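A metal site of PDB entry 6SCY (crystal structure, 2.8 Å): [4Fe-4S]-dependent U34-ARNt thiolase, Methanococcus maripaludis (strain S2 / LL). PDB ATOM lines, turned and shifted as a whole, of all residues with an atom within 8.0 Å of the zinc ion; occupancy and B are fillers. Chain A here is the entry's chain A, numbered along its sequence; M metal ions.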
ATOM      1  N   LYS A   5      26.741  12.835  33.954  1.00  0.00           N
ATOM      2  CA  LYS A   5      27.782  12.267  33.101  1.00  0.00           C
ATOM      3  C   LYS A   5      27.286  11.120  32.216  1.00  0.00           C
ATOM      4  O   LYS A   5      26.373  10.392  32.609  1.00  0.00           O
ATOM      5  CB  LYS A   5      29.014  11.867  33.935  1.00  0.00           C
ATOM      6  CG  LYS A   5      28.781  10.831  35.038  1.00  0.00           C
ATOM      7  CD  LYS A   5      30.098  10.433  35.729  1.00  0.00           C
ATOM      8  CE  LYS A   5      30.657  11.503  36.648  1.00  0.00           C
ATOM      9  NZ  LYS A   5      31.974  11.106  37.208  1.00  0.00           N
ATOM     10  N   CYS A   6      27.854  11.001  31.004  1.00  0.00           N
ATOM     11  CA  CYS A   6      27.532  10.007  29.990  1.00  0.00           C
ATOM     12  C   CYS A   6      27.664   8.572  30.534  1.00  0.00           C
ATOM     13  O   CYS A   6      28.634   8.264  31.212  1.00  0.00           O
ATOM     14  CB  CYS A   6      28.407  10.211  28.754  1.00  0.00           C
ATOM     15  SG  CYS A   6      27.971   9.158  27.352  1.00  0.00           S
ATOM     16  N   ARG A   7      26.671   7.706  30.230  1.00  0.00           N
ATOM     17  CA  ARG A   7      26.644   6.300  30.670  1.00  0.00           C
ATOM     18  C   ARG A   7      27.803   5.461  30.087  1.00  0.00           C
ATOM     19  O   ARG A   7      28.266   4.530  30.763  1.00  0.00           O
ATOM     20  CB  ARG A   7      25.270   5.664  30.348  1.00  0.00           C
ATOM     21  CG  ARG A   7      25.084   4.270  30.965  1.00  0.00           C
ATOM     22  CD  ARG A   7      24.737   3.183  29.945  1.00  0.00           C
ATOM     23  NE  ARG A   7      25.744   2.125  29.887  1.00  0.00           N
ATOM     24  CZ  ARG A   7      25.490   0.847  29.636  1.00  0.00           C
ATOM     25  NH1 ARG A   7      24.251   0.430  29.434  1.00  0.00           N
ATOM     26  NH2 ARG A   7      26.484  -0.038  29.598  1.00  0.00           N
ATOM     27  N   LYS A   8      28.289   5.807  28.878  1.00  0.00           N
ATOM     28  CA  LYS A   8      29.358   5.068  28.189  1.00  0.00           C
ATOM     29  C   LYS A   8      30.779   5.619  28.383  1.00  0.00           C
ATOM     30  O   LYS A   8      31.728   4.829  28.283  1.00  0.00           O
ATOM     31  CB  LYS A   8      29.048   4.924  26.696  1.00  0.00           C
ATOM     32  CG  LYS A   8      27.944   3.918  26.382  1.00  0.00           C
ATOM     33  CD  LYS A   8      28.441   2.468  26.355  1.00  0.00           C
ATOM     34  CE  LYS A   8      27.503   1.558  25.598  1.00  0.00           C
ATOM     35  NZ  LYS A   8      28.022   0.166  25.519  1.00  0.00           N
ATOM     36  N   CYS A   9      30.948   6.931  28.634  1.00  0.00           N
ATOM     37  CA  CYS A   9      32.283   7.529  28.784  1.00  0.00           C
ATOM     38  C   CYS A   9      32.433   8.518  29.965  1.00  0.00           C
ATOM     39  O   CYS A   9      33.522   9.044  30.170  1.00  0.00           O
ATOM     40  CB  CYS A   9      32.732   8.164  27.469  1.00  0.00           C
ATOM     41  SG  CYS A   9      31.807   9.652  27.007  1.00  0.00           S
ATOM     42  N   GLY A  10      31.354   8.756  30.703  1.00  0.00           N
ATOM     43  CA  GLY A  10      31.330   9.665  31.858  1.00  0.00           C
ATOM     44  C   GLY A  10      31.552  11.139  31.572  1.00  0.00           C
ATOM     45  O   GLY A  10      31.915  11.890  32.490  1.00  0.00           O
ATOM     46  N   LYS A  11      31.353  11.569  30.310  1.00  0.00           N
ATOM     47  CA  LYS A  11      31.554  12.947  29.871  1.00  0.00           C
ATOM     48  C   LYS A  11      30.253  13.755  29.888  1.00  0.00           C
ATOM     49  O   LYS A  11      29.197  13.140  29.790  1.00  0.00           O
ATOM     50  CB  LYS A  11      32.200  12.961  28.470  1.00  0.00           C
ATOM     51  CG  LYS A  11      33.665  13.382  28.474  1.00  0.00           C
ATOM     52  CD  LYS A  11      34.625  12.424  29.208  1.00  0.00           C
ATOM     53  CE  LYS A  11      35.995  13.034  29.451  1.00  0.00           C
ATOM     54  NZ  LYS A  11      36.620  12.487  30.673  1.00  0.00           N
ATOM     55  N   PRO A  12      30.280  15.122  29.986  1.00  0.00           N
ATOM     56  CA  PRO A  12      29.012  15.868  29.963  1.00  0.00           C
ATOM     57  C   PRO A  12      28.090  15.437  28.835  1.00  0.00           C
ATOM     58  O   PRO A  12      28.556  15.185  27.718  1.00  0.00           O
ATOM     59  CB  PRO A  12      29.468  17.324  29.839  1.00  0.00           C
ATOM     60  CG  PRO A  12      30.810  17.345  30.469  1.00  0.00           C
ATOM     61  CD  PRO A  12      31.434  16.024  30.128  1.00  0.00           C
ATOM     62  N   SER A  13      26.813  15.274  29.149  1.00  0.00           N
ATOM     63  CA  SER A  13      25.785  14.750  28.252  1.00  0.00           C
ATOM     64  C   SER A  13      24.951  15.793  27.500  1.00  0.00           C
ATOM     65  O   SER A  13      24.814  16.935  27.948  1.00  0.00           O
ATOM     66  CB  SER A  13      24.868  13.818  29.045  1.00  0.00           C
ATOM     67  OG  SER A  13      23.946  13.139  28.226  1.00  0.00           O
ATOM     68  N   ASN A  23      22.147   8.854  30.261  1.00  0.00           N
ATOM     69  CA  ASN A  23      22.626  10.094  29.665  1.00  0.00           C
ATOM     70  C   ASN A  23      23.688   9.790  28.615  1.00  0.00           C
ATOM     71  O   ASN A  23      24.544   8.928  28.842  1.00  0.00           O
ATOM     72  CB  ASN A  23      23.173  11.001  30.762  1.00  0.00           C
ATOM     73  CG  ASN A  23      22.158  11.407  31.821  1.00  0.00           C
ATOM     74  OD1 ASN A  23      21.010  11.752  31.531  1.00  0.00           O
ATOM     75  ND2 ASN A  23      22.568  11.385  33.069  1.00  0.00           N
ATOM     76  N   TYR A  24      23.605  10.450  27.440  1.00  0.00           N
ATOM     77  CA  TYR A  24      24.538  10.266  26.324  1.00  0.00           C
ATOM     78  C   TYR A  24      24.968  11.581  25.698  1.00  0.00           C
ATOM     79  O   TYR A  24      24.123  12.434  25.401  1.00  0.00           O
ATOM     80  CB  TYR A  24      23.933   9.371  25.228  1.00  0.00           C
ATOM     81  CG  TYR A  24      23.530   7.988  25.671  1.00  0.00           C
ATOM     82  CD1 TYR A  24      24.487   7.013  25.910  1.00  0.00           C
ATOM     83  CD2 TYR A  24      22.193   7.635  25.798  1.00  0.00           C
ATOM     84  CE1 TYR A  24      24.125   5.720  26.301  1.00  0.00           C
ATOM     85  CE2 TYR A  24      21.817   6.343  26.186  1.00  0.00           C
ATOM     86  CZ  TYR A  24      22.788   5.395  26.438  1.00  0.00           C
ATOM     87  OH  TYR A  24      22.427   4.128  26.814  1.00  0.00           O
ATOM     88  N   CYS A  25      26.270  11.733  25.449  1.00  0.00           N
ATOM     89  CA  CYS A  25      26.838  12.894  24.764  1.00  0.00           C
ATOM     90  C   CYS A  25      26.576  12.708  23.265  1.00  0.00           C
ATOM     91  O   CYS A  25      25.975  11.693  22.893  1.00  0.00           O
ATOM     92  CB  CYS A  25      28.332  13.010  25.054  1.00  0.00           C
ATOM     93  SG  CYS A  25      29.309  11.584  24.514  1.00  0.00           S
ATOM     94  N   LYS A  26      26.998  13.651  22.395  1.00  0.00           N
ATOM     95  CA  LYS A  26      26.771  13.544  20.940  1.00  0.00           C
ATOM     96  C   LYS A  26      27.288  12.218  20.370  1.00  0.00           C
ATOM     97  O   LYS A  26      26.508  11.455  19.825  1.00  0.00           O
ATOM     98  CB  LYS A  26      27.383  14.764  20.203  1.00  0.00           C
ATOM     99  CG  LYS A  26      27.030  14.847  18.728  1.00  0.00           C
ATOM    100  CD  LYS A  26      27.784  15.967  18.020  1.00  0.00           C
ATOM    101  CE  LYS A  26      27.522  15.979  16.530  1.00  0.00           C
ATOM    102  NZ  LYS A  26      28.242  17.087  15.861  1.00  0.00           N
ATOM    103  N   GLU A  27      28.596  11.939  20.568  1.00  0.00           N
ATOM    104  CA  GLU A  27      29.320  10.763  20.065  1.00  0.00           C
ATOM    105  C   GLU A  27      28.768   9.437  20.541  1.00  0.00           C
ATOM    106  O   GLU A  27      28.705   8.511  19.740  1.00  0.00           O
ATOM    107  CB  GLU A  27      30.815  10.846  20.391  1.00  0.00           C
ATOM    108  CG  GLU A  27      31.497  12.087  19.838  1.00  0.00           C
ATOM    109  CD  GLU A  27      31.893  13.099  20.888  1.00  0.00           C
ATOM    110  OE1 GLU A  27      31.012  13.554  21.649  1.00  0.00           O
ATOM    111  OE2 GLU A  27      33.102  13.437  20.948  1.00  0.00           O
ATOM    112  N   CYS A  28      28.394   9.335  21.830  1.00  0.00           N
ATOM    113  CA  CYS A  28      27.843   8.099  22.419  1.00  0.00           C
ATOM    114  C   CYS A  28      26.392   7.866  22.029  1.00  0.00           C
ATOM    115  O   CYS A  28      25.962   6.717  22.017  1.00  0.00           O
ATOM    116  CB  CYS A  28      28.016   8.082  23.935  1.00  0.00           C
ATOM    117  SG  CYS A  28      29.736   7.899  24.474  1.00  0.00           S
ATOM    118  N   PHE A  29      25.646   8.941  21.718  1.00  0.00           N
ATOM    119  CA  PHE A  29      24.250   8.808  21.307  1.00  0.00           C
ATOM    120  C   PHE A  29      24.183   8.267  19.875  1.00  0.00           C
ATOM    121  O   PHE A  29      23.449   7.316  19.612  1.00  0.00           O
ATOM    122  CB  PHE A  29      23.486  10.124  21.485  1.00  0.00           C
ATOM    123  CG  PHE A  29      22.087  10.104  20.923  1.00  0.00           C
ATOM    124  CD1 PHE A  29      21.072   9.394  21.560  1.00  0.00           C
ATOM    125  CD2 PHE A  29      21.785  10.763  19.740  1.00  0.00           C
ATOM    126  CE1 PHE A  29      19.790   9.352  21.021  1.00  0.00           C
ATOM    127  CE2 PHE A  29      20.503  10.712  19.197  1.00  0.00           C
ATOM    128  CZ  PHE A  29      19.515  10.008  19.845  1.00  0.00           C
ATOM    129  N   LYS A  31      26.479   6.537  18.320  1.00  0.00           N
ATOM    130  CA  LYS A  31      27.005   5.182  18.418  1.00  0.00           C
ATOM    131  C   LYS A  31      25.943   4.194  18.914  1.00  0.00           C
ATOM    132  O   LYS A  31      25.930   3.061  18.421  1.00  0.00           O
ATOM    133  CB  LYS A  31      28.197   5.169  19.361  1.00  0.00           C
ATOM    134  CG  LYS A  31      29.253   4.118  19.050  1.00  0.00           C
ATOM    135  CD  LYS A  31      30.364   4.098  20.120  1.00  0.00           C
ATOM    136  CE  LYS A  31      29.987   3.349  21.392  1.00  0.00           C
ATOM    137  NZ  LYS A  31      30.868   3.715  22.533  1.00  0.00           N
HETATM  138 ZN    ZN M   1      29.804   9.329  26.116  1.00  0.00          ZN
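The backbone NH (N) of Cys 28 is in hydrogen-bond range of the side-chain sulfur (SG) of Cys 25, at 3.6 Å. N of Cys 25 sits close to SG of Cys 6. SG of Cys 6 lies close to N of Lys 8 (3.7 Å). O of Lys 11 lies within hydrogen-bond range of N of Cys 6, 2.8 Å away. The side-chain sulfur (SG) of Cys 6 lies close to the backbone carbonyl oxygen (O) of Asn 23 (3.7 Å).
The zinc ion is bound by SG of Cys 28 (2.2 Å), SG of Cys 9 (2.2 Å) and SG of Cys 6 (2.2 Å). The zinc ion has three donor atoms within binding distance. Slightly farther from the zinc ion lies the side-chain sulfur (SG) of Cys 25 (2.8 Å).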
